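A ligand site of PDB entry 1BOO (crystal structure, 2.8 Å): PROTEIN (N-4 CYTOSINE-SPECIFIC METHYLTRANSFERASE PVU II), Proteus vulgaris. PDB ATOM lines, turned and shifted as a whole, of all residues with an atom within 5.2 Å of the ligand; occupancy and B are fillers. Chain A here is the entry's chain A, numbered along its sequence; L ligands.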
ATOM      1  N   GLY A  20       4.852 -12.754  22.407  1.00  0.00           N
ATOM      2  CA  GLY A  20       5.511 -13.516  23.452  1.00  0.00           C
ATOM      3  C   GLY A  20       6.741 -12.867  24.039  1.00  0.00           C
ATOM      4  O   GLY A  20       7.094 -11.719  23.710  1.00  0.00           O
ATOM      5  N   ASP A  21       7.390 -13.590  24.953  1.00  0.00           N
ATOM      6  CA  ASP A  21       8.583 -13.088  25.594  1.00  0.00           C
ATOM      7  C   ASP A  21       9.791 -13.444  24.717  1.00  0.00           C
ATOM      8  O   ASP A  21      10.078 -14.631  24.503  1.00  0.00           O
ATOM      9  CB  ASP A  21       8.719 -13.744  26.973  1.00  0.00           C
ATOM     10  CG  ASP A  21       9.941 -13.266  27.750  1.00  0.00           C
ATOM     11  OD1 ASP A  21      10.640 -12.319  27.307  1.00  0.00           O
ATOM     12  OD2 ASP A  21      10.184 -13.856  28.818  1.00  0.00           O
ATOM     13  N   SER A  22      10.518 -12.435  24.257  1.00  0.00           N
ATOM     14  CA  SER A  22      11.677 -12.682  23.393  1.00  0.00           C
ATOM     15  C   SER A  22      12.845 -13.410  24.058  1.00  0.00           C
ATOM     16  O   SER A  22      13.581 -14.116  23.374  1.00  0.00           O
ATOM     17  CB  SER A  22      12.129 -11.403  22.690  1.00  0.00           C
ATOM     18  OG  SER A  22      12.539 -10.452  23.635  1.00  0.00           O
ATOM     19  N   SER A  40      15.050  -1.214  19.882  1.00  0.00           N
ATOM     20  CA  SER A  40      15.100  -0.069  20.781  1.00  0.00           C
ATOM     21  C   SER A  40      14.207  -0.524  21.946  1.00  0.00           C
ATOM     22  O   SER A  40      12.992  -0.559  21.832  1.00  0.00           O
ATOM     23  CB  SER A  40      14.580   1.214  20.134  1.00  0.00           C
ATOM     24  OG  SER A  40      13.217   1.132  19.820  1.00  0.00           O
ATOM     25  N   PRO A  41      14.822  -1.005  23.050  1.00  0.00           N
ATOM     26  CA  PRO A  41      14.149  -1.484  24.253  1.00  0.00           C
ATOM     27  C   PRO A  41      13.091  -0.568  24.896  1.00  0.00           C
ATOM     28  O   PRO A  41      13.131   0.647  24.735  1.00  0.00           O
ATOM     29  CB  PRO A  41      15.330  -1.733  25.191  1.00  0.00           C
ATOM     30  CG  PRO A  41      16.369  -2.216  24.259  1.00  0.00           C
ATOM     31  CD  PRO A  41      16.269  -1.170  23.185  1.00  0.00           C
ATOM     32  N   PRO A  42      12.120  -1.167  25.617  1.00  0.00           N
ATOM     33  CA  PRO A  42      11.061  -0.449  26.295  1.00  0.00           C
ATOM     34  C   PRO A  42      11.627   0.186  27.588  1.00  0.00           C
ATOM     35  O   PRO A  42      12.150  -0.517  28.443  1.00  0.00           O
ATOM     36  CB  PRO A  42      10.101  -1.572  26.631  1.00  0.00           C
ATOM     37  CG  PRO A  42      11.044  -2.639  27.039  1.00  0.00           C
ATOM     38  CD  PRO A  42      11.974  -2.610  25.871  1.00  0.00           C
ATOM     39  N   TRP A  62      18.352  -6.803  33.541  1.00  0.00           N
ATOM     40  CA  TRP A  62      17.233  -7.277  32.738  1.00  0.00           C
ATOM     41  C   TRP A  62      17.646  -7.362  31.277  1.00  0.00           C
ATOM     42  O   TRP A  62      17.523  -8.407  30.645  1.00  0.00           O
ATOM     43  CB  TRP A  62      16.059  -6.293  32.886  1.00  0.00           C
ATOM     44  CG  TRP A  62      14.940  -6.501  31.921  1.00  0.00           C
ATOM     45  CD1 TRP A  62      13.939  -7.409  32.027  1.00  0.00           C
ATOM     46  CD2 TRP A  62      14.700  -5.756  30.725  1.00  0.00           C
ATOM     47  NE1 TRP A  62      13.068  -7.271  30.978  1.00  0.00           N
ATOM     48  CE2 TRP A  62      13.509  -6.263  30.163  1.00  0.00           C
ATOM     49  CE3 TRP A  62      15.363  -4.712  30.079  1.00  0.00           C
ATOM     50  CZ2 TRP A  62      12.970  -5.743  28.978  1.00  0.00           C
ATOM     51  CZ3 TRP A  62      14.824  -4.208  28.906  1.00  0.00           C
ATOM     52  CH2 TRP A  62      13.631  -4.733  28.369  1.00  0.00           C
ATOM     53  N   PHE A  66      19.003 -10.573  27.667  1.00  0.00           N
ATOM     54  CA  PHE A  66      18.716 -10.653  26.251  1.00  0.00           C
ATOM     55  C   PHE A  66      20.024 -10.560  25.493  1.00  0.00           C
ATOM     56  O   PHE A  66      20.265 -11.336  24.575  1.00  0.00           O
ATOM     57  CB  PHE A  66      17.761  -9.551  25.840  1.00  0.00           C
ATOM     58  CG  PHE A  66      16.427  -9.608  26.529  1.00  0.00           C
ATOM     59  CD1 PHE A  66      16.256  -9.032  27.783  1.00  0.00           C
ATOM     60  CD2 PHE A  66      15.337 -10.200  25.920  1.00  0.00           C
ATOM     61  CE1 PHE A  66      15.015  -9.038  28.424  1.00  0.00           C
ATOM     62  CE2 PHE A  66      14.088 -10.212  26.538  1.00  0.00           C
ATOM     63  CZ  PHE A  66      13.926  -9.621  27.794  1.00  0.00           C
ATOM     64  N   HIS A 233       1.285   2.883  18.407  1.00  0.00           N
ATOM     65  CA  HIS A 233       2.341   2.641  19.385  1.00  0.00           C
ATOM     66  C   HIS A 233       2.873   3.949  19.992  1.00  0.00           C
ATOM     67  O   HIS A 233       3.323   4.840  19.254  1.00  0.00           O
ATOM     68  CB  HIS A 233       3.498   1.833  18.788  1.00  0.00           C
ATOM     69  CG  HIS A 233       4.438   1.280  19.818  1.00  0.00           C
ATOM     70  ND1 HIS A 233       5.213   2.093  20.618  1.00  0.00           N
ATOM     71  CD2 HIS A 233       4.633   0.020  20.273  1.00  0.00           C
ATOM     72  CE1 HIS A 233       5.834   1.362  21.520  1.00  0.00           C
ATOM     73  NE2 HIS A 233       5.489   0.094  21.337  1.00  0.00           N
ATOM     74  N   ALA A 235       5.636   4.702  21.494  1.00  0.00           N
ATOM     75  CA  ALA A 235       7.014   5.037  21.194  1.00  0.00           C
ATOM     76  C   ALA A 235       7.612   4.149  20.098  1.00  0.00           C
ATOM     77  O   ALA A 235       8.066   3.048  20.385  1.00  0.00           O
ATOM     78  CB  ALA A 235       7.843   4.938  22.446  1.00  0.00           C
ATOM     79  N   ARG A 236       7.596   4.625  18.846  1.00  0.00           N
ATOM     80  CA  ARG A 236       8.119   3.881  17.707  1.00  0.00           C
ATOM     81  C   ARG A 236       9.103   4.777  16.967  1.00  0.00           C
ATOM     82  O   ARG A 236       8.979   6.012  17.031  1.00  0.00           O
ATOM     83  CB  ARG A 236       6.969   3.464  16.781  1.00  0.00           C
ATOM     84  CG  ARG A 236       6.154   4.639  16.235  1.00  0.00           C
ATOM     85  CD  ARG A 236       4.959   4.158  15.389  1.00  0.00           C
ATOM     86  NE  ARG A 236       4.298   5.247  14.665  1.00  0.00           N
ATOM     87  CZ  ARG A 236       3.720   6.302  15.250  1.00  0.00           C
ATOM     88  NH1 ARG A 236       3.681   6.420  16.577  1.00  0.00           N
ATOM     89  NH2 ARG A 236       3.241   7.275  14.490  1.00  0.00           N
ATOM     90  N   PHE A 237      10.058   4.178  16.247  1.00  0.00           N
ATOM     91  CA  PHE A 237      11.057   4.965  15.527  1.00  0.00           C
ATOM     92  C   PHE A 237      10.797   5.071  14.027  1.00  0.00           C
ATOM     93  O   PHE A 237      10.111   4.218  13.458  1.00  0.00           O
ATOM     94  CB  PHE A 237      12.503   4.508  15.856  1.00  0.00           C
ATOM     95  CG  PHE A 237      12.800   3.039  15.615  1.00  0.00           C
ATOM     96  CD1 PHE A 237      12.288   2.352  14.520  1.00  0.00           C
ATOM     97  CD2 PHE A 237      13.624   2.343  16.483  1.00  0.00           C
ATOM     98  CE1 PHE A 237      12.605   1.001  14.320  1.00  0.00           C
ATOM     99  CE2 PHE A 237      13.930   0.999  16.276  1.00  0.00           C
ATOM    100  CZ  PHE A 237      13.426   0.324  15.198  1.00  0.00           C
ATOM    101  N   ASP A 258      14.022  -8.495  15.396  1.00  0.00           N
ATOM    102  CA  ASP A 258      13.740  -7.345  16.280  1.00  0.00           C
ATOM    103  C   ASP A 258      13.077  -7.910  17.536  1.00  0.00           C
ATOM    104  O   ASP A 258      11.928  -8.323  17.501  1.00  0.00           O
ATOM    105  CB  ASP A 258      12.841  -6.341  15.573  1.00  0.00           C
ATOM    106  CG  ASP A 258      12.618  -5.079  16.407  1.00  0.00           C
ATOM    107  OD1 ASP A 258      12.571  -5.172  17.652  1.00  0.00           O
ATOM    108  OD2 ASP A 258      12.470  -3.987  15.794  1.00  0.00           O
ATOM    109  N   ILE A 259      13.794  -7.932  18.639  1.00  0.00           N
ATOM    110  CA  ILE A 259      13.266  -8.518  19.868  1.00  0.00           C
ATOM    111  C   ILE A 259      12.226  -7.744  20.721  1.00  0.00           C
ATOM    112  O   ILE A 259      11.782  -8.248  21.762  1.00  0.00           O
ATOM    113  CB  ILE A 259      14.405  -9.024  20.778  1.00  0.00           C
ATOM    114  CG1 ILE A 259      15.444  -7.919  20.971  1.00  0.00           C
ATOM    115  CG2 ILE A 259      15.058 -10.255  20.160  1.00  0.00           C
ATOM    116  CD1 ILE A 259      16.469  -8.275  22.030  1.00  0.00           C
ATOM    117  N   PHE A 260      11.889  -6.522  20.297  1.00  0.00           N
ATOM    118  CA  PHE A 260      10.892  -5.677  20.978  1.00  0.00           C
ATOM    119  C   PHE A 260      10.139  -5.007  19.825  1.00  0.00           C
ATOM    120  O   PHE A 260      10.112  -3.785  19.724  1.00  0.00           O
ATOM    121  CB  PHE A 260      11.563  -4.620  21.870  1.00  0.00           C
ATOM    122  CG  PHE A 260      12.436  -5.187  22.963  1.00  0.00           C
ATOM    123  CD1 PHE A 260      11.942  -6.110  23.858  1.00  0.00           C
ATOM    124  CD2 PHE A 260      13.749  -4.802  23.081  1.00  0.00           C
ATOM    125  CE1 PHE A 260      12.754  -6.645  24.842  1.00  0.00           C
ATOM    126  CE2 PHE A 260      14.561  -5.336  24.065  1.00  0.00           C
ATOM    127  CZ  PHE A 260      14.058  -6.258  24.945  1.00  0.00           C
ATOM    128  N   GLY A 261       9.519  -5.817  18.982  1.00  0.00           N
ATOM    129  CA  GLY A 261       8.830  -5.339  17.807  1.00  0.00           C
ATOM    130  C   GLY A 261       8.034  -4.062  17.816  1.00  0.00           C
ATOM    131  O   GLY A 261       8.210  -3.223  16.937  1.00  0.00           O
ATOM    132  N   GLY A 262       7.116  -3.938  18.771  1.00  0.00           N
ATOM    133  CA  GLY A 262       6.289  -2.735  18.831  1.00  0.00           C
ATOM    134  C   GLY A 262       5.412  -2.694  17.602  1.00  0.00           C
ATOM    135  O   GLY A 262       4.683  -3.650  17.331  1.00  0.00           O
ATOM    136  N   SER A 263       5.512  -1.625  16.829  1.00  0.00           N
ATOM    137  CA  SER A 263       4.708  -1.503  15.627  1.00  0.00           C
ATOM    138  C   SER A 263       5.327  -2.229  14.413  1.00  0.00           C
ATOM    139  O   SER A 263       4.791  -2.201  13.306  1.00  0.00           O
ATOM    140  CB  SER A 263       4.404  -0.038  15.328  1.00  0.00           C
ATOM    141  OG  SER A 263       5.574   0.757  15.207  1.00  0.00           O
ATOM    142  N   ASN A 264       6.465  -2.897  14.639  1.00  0.00           N
ATOM    143  CA  ASN A 264       7.179  -3.663  13.607  1.00  0.00           C
ATOM    144  C   ASN A 264       7.709  -2.878  12.443  1.00  0.00           C
ATOM    145  O   ASN A 264       7.660  -3.368  11.318  1.00  0.00           O
ATOM    146  CB  ASN A 264       6.316  -4.803  13.088  1.00  0.00           C
ATOM    147  CG  ASN A 264       7.134  -5.910  12.452  1.00  0.00           C
ATOM    148  OD1 ASN A 264       8.292  -6.158  12.807  1.00  0.00           O
ATOM    149  ND2 ASN A 264       6.525  -6.591  11.514  1.00  0.00           N
ATOM    150  N   THR A 265       8.213  -1.678  12.688  1.00  0.00           N
ATOM    151  CA  THR A 265       8.790  -0.854  11.627  1.00  0.00           C
ATOM    152  C   THR A 265       9.924  -1.645  10.952  1.00  0.00           C
ATOM    153  O   THR A 265      10.086  -1.631   9.720  1.00  0.00           O
ATOM    154  CB  THR A 265       9.389   0.415  12.199  1.00  0.00           C
ATOM    155  OG1 THR A 265       8.360   1.159  12.862  1.00  0.00           O
ATOM    156  CG2 THR A 265       9.978   1.252  11.106  1.00  0.00           C
ATOM    157  N   THR A 266      10.683  -2.362  11.776  1.00  0.00           N
ATOM    158  CA  THR A 266      11.808  -3.160  11.293  1.00  0.00           C
ATOM    159  C   THR A 266      11.339  -4.123  10.247  1.00  0.00           C
ATOM    160  O   THR A 266      11.604  -3.916   9.074  1.00  0.00           O
ATOM    161  CB  THR A 266      12.506  -3.914  12.450  1.00  0.00           C
ATOM    162  OG1 THR A 266      12.651  -3.037  13.576  1.00  0.00           O
ATOM    163  CG2 THR A 266      13.879  -4.389  12.001  1.00  0.00           C
ATOM    164  N   PHE A 280       9.470 -10.192  17.684  1.00  0.00           N
ATOM    165  CA  PHE A 280       8.800 -10.698  18.870  1.00  0.00           C
ATOM    166  C   PHE A 280       8.278  -9.465  19.593  1.00  0.00           C
ATOM    167  O   PHE A 280       8.974  -8.429  19.637  1.00  0.00           O
ATOM    168  CB  PHE A 280       9.772 -11.425  19.783  1.00  0.00           C
ATOM    169  CG  PHE A 280      10.572 -12.476  19.089  1.00  0.00           C
ATOM    170  CD1 PHE A 280       9.967 -13.425  18.277  1.00  0.00           C
ATOM    171  CD2 PHE A 280      11.948 -12.553  19.274  1.00  0.00           C
ATOM    172  CE1 PHE A 280      10.704 -14.421  17.672  1.00  0.00           C
ATOM    173  CE2 PHE A 280      12.684 -13.544  18.677  1.00  0.00           C
ATOM    174  CZ  PHE A 280      12.057 -14.483  17.879  1.00  0.00           C
ATOM    175  N   GLU A 281       7.045  -9.544  20.088  1.00  0.00           N
ATOM    176  CA  GLU A 281       6.437  -8.444  20.849  1.00  0.00           C
ATOM    177  C   GLU A 281       5.530  -9.081  21.871  1.00  0.00           C
ATOM    178  O   GLU A 281       4.896 -10.085  21.586  1.00  0.00           O
ATOM    179  CB  GLU A 281       5.634  -7.526  19.943  1.00  0.00           C
ATOM    180  CG  GLU A 281       4.708  -6.573  20.654  1.00  0.00           C
ATOM    181  CD  GLU A 281       5.420  -5.675  21.633  1.00  0.00           C
ATOM    182  OE1 GLU A 281       6.350  -4.954  21.242  1.00  0.00           O
ATOM    183  OE2 GLU A 281       5.031  -5.678  22.810  1.00  0.00           O
ATOM    184  N   MET A 282       5.485  -8.509  23.071  1.00  0.00           N
ATOM    185  CA  MET A 282       4.669  -9.065  24.135  1.00  0.00           C
ATOM    186  C   MET A 282       3.172  -8.723  24.087  1.00  0.00           C
ATOM    187  O   MET A 282       2.328  -9.563  24.403  1.00  0.00           O
ATOM    188  CB  MET A 282       5.255  -8.658  25.476  1.00  0.00           C
ATOM    189  CG  MET A 282       5.321  -9.792  26.447  1.00  0.00           C
ATOM    190  SD  MET A 282       6.478  -9.435  27.746  1.00  0.00           S
ATOM    191  CE  MET A 282       5.719 -10.355  29.077  1.00  0.00           C
ATOM    192  N   LYS A 283       2.851  -7.483  23.703  1.00  0.00           N
ATOM    193  CA  LYS A 283       1.468  -7.015  23.640  1.00  0.00           C
ATOM    194  C   LYS A 283       0.773  -7.287  22.296  1.00  0.00           C
ATOM    195  O   LYS A 283       1.211  -6.810  21.236  1.00  0.00           O
ATOM    196  CB  LYS A 283       1.384  -5.525  23.946  1.00  0.00           C
ATOM    197  CG  LYS A 283       1.941  -5.133  25.282  1.00  0.00           C
ATOM    198  CD  LYS A 283       1.670  -3.677  25.573  1.00  0.00           C
ATOM    199  CE  LYS A 283       0.254  -3.522  26.043  1.00  0.00           C
ATOM    200  NZ  LYS A 283      -0.112  -2.096  26.292  1.00  0.00           N
ATOM    201  N   TYR A 286      -0.258  -4.353  19.874  1.00  0.00           N
ATOM    202  CA  TYR A 286       0.827  -3.842  19.071  1.00  0.00           C
ATOM    203  C   TYR A 286       1.023  -4.707  17.849  1.00  0.00           C
ATOM    204  O   TYR A 286       1.082  -4.194  16.732  1.00  0.00           O
ATOM    205  CB  TYR A 286       2.076  -3.758  19.921  1.00  0.00           C
ATOM    206  CG  TYR A 286       2.024  -2.679  20.980  1.00  0.00           C
ATOM    207  CD1 TYR A 286       1.099  -1.653  20.920  1.00  0.00           C
ATOM    208  CD2 TYR A 286       2.946  -2.670  22.027  1.00  0.00           C
ATOM    209  CE1 TYR A 286       1.091  -0.628  21.874  1.00  0.00           C
ATOM    210  CE2 TYR A 286       2.956  -1.630  22.985  1.00  0.00           C
ATOM    211  CZ  TYR A 286       2.014  -0.609  22.901  1.00  0.00           C
ATOM    212  OH  TYR A 286       2.062   0.445  23.779  1.00  0.00           O
HETATM  213  N1  LIG L   1      10.982  -0.080  17.444  1.00  0.00           N
HETATM  214  C1  LIG L   1       9.627  -0.345  17.770  1.00  0.00           C
HETATM  215  C2  LIG L   1       9.254   0.167  19.169  1.00  0.00           C
HETATM  216  C3  LIG L   1       9.393  -0.887  20.267  1.00  0.00           C
HETATM  217  S1  LIG L   1       9.221  -0.138  21.920  1.00  0.00           S
HETATM  218  C4  LIG L   1       8.657   0.204  16.752  1.00  0.00           C
HETATM  219  O1  LIG L   1       9.000   1.208  16.013  1.00  0.00           O
HETATM  220  O2  LIG L   1       7.429   0.187  17.163  1.00  0.00           O
HETATM  221  C5  LIG L   1       9.620  -1.596  22.981  1.00  0.00           C
HETATM  222  C6  LIG L   1       8.681  -2.631  22.751  1.00  0.00           C
HETATM  223  O3  LIG L   1       9.076  -3.782  23.556  1.00  0.00           O
HETATM  224  C7  LIG L   1       7.346  -2.321  23.430  1.00  0.00           C
HETATM  225  O4  LIG L   1       6.186  -2.446  22.510  1.00  0.00           O
HETATM  226  C8  LIG L   1       7.202  -3.525  24.523  1.00  0.00           C
HETATM  227  O5  LIG L   1       5.816  -3.896  24.724  1.00  0.00           O
HETATM  228  C9  LIG L   1       7.950  -4.661  23.899  1.00  0.00           C
HETATM  229  N2  LIG L   1       8.399  -5.612  24.940  1.00  0.00           N
HETATM  230  C10 LIG L   1       8.795  -5.376  26.280  1.00  0.00           C
HETATM  231  N3  LIG L   1       9.337  -6.466  26.886  1.00  0.00           N
HETATM  232  C11 LIG L   1       9.281  -7.416  25.929  1.00  0.00           C
HETATM  233  C12 LIG L   1       9.704  -8.654  25.999  1.00  0.00           C
HETATM  234  N4  LIG L   1      10.322  -9.131  27.075  1.00  0.00           N
HETATM  235  N5  LIG L   1       9.557  -9.401  24.914  1.00  0.00           N
HETATM  236  C13 LIG L   1       8.989  -8.857  23.795  1.00  0.00           C
HETATM  237  N6  LIG L   1       8.521  -7.622  23.570  1.00  0.00           N
HETATM  238  C14 LIG L   1       8.725  -6.964  24.754  1.00  0.00           C
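N of Ser 263 lies within hydrogen-bond range of O2 of the ligand, at 2.7 Å. An oxygen (O2) of the ligand is in hydrogen-bond range of the side-chain hydroxyl (OG) of Ser 263. OE2 of Glu 281 lies within hydrogen-bond range of O5 of the ligand (2.7 Å). An oxygen (O4) of the ligand sits at hydrogen-bond distance from a ring nitrogen (NE2) of His 233, 2.9 Å away. N of Phe 237 lies within hydrogen-bond range of O1 of the ligand. N of Met 282 is in hydrogen-bond range of N6 of the ligand, at 3.2 Å. The side-chain carboxylate (OD1) of Asp 21 is in hydrogen-bond range of a nitrogen (N4) of the ligand (3.2 Å). An oxygen (O1) of the ligand is in hydrogen-bond range of the side-chain hydroxyl (OG1) of Thr 265. The backbone NH of Ser 22 lies within hydrogen-bond range of a nitrogen (N5) of the ligand. OG of Ser 22 lies within hydrogen-bond range of N5 of the ligand, 3.4 Å away. The side-chain hydroxyl (OG) of Ser 40 sits at hydrogen-bond distance from a nitrogen (N1) of the ligand (3.5 Å).
O of Glu 281 is in hydrogen-bond range of N of Gly 20, at 2.8 Å. The backbone NH of Gly 262 lies within hydrogen-bond range of the side-chain carboxylate of Glu 281, 2.8 Å away. The side-chain carboxylate (OE2) of Glu 281 lies within hydrogen-bond range of the backbone NH (N) of Lys 283 (3.0 Å). The guanidinium group of Arg 236 sits at hydrogen-bond distance from the backbone carbonyl oxygen of His 233 (3.1 Å). A ring nitrogen (ND1) of His 233 is in hydrogen-bond range of the backbone NH of Ala 235, at 2.8 Å. The backbone NH (N) of Phe 260 lies within hydrogen-bond range of the side-chain carboxylate (OD1) of Asp 258, 3.0 Å away. OG of Ser 22 is in hydrogen-bond range of O of Ile 259, 3.0 Å away. The backbone NH (N) of Gly 261 is in hydrogen-bond range of the side-chain carboxylate (OD1) of Asp 258.
S1 of the ligand sits close to O of Ala 235 (3.7 Å). Residues that only touch the ligand: Gly 20 (3.4 Å), Pro 42 (3.6 Å), Phe 66 (3.7 Å), Arg 236 (3.1 Å), Ile 259 (3.5 Å), Phe 260 (3.0 Å), Gly 261 (3.3 Å), Gly 262 (3.5 Å) and Tyr 286 (3.3 Å). Along chain A the residues within 4 Å of the ligand span positions 20 to 286.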
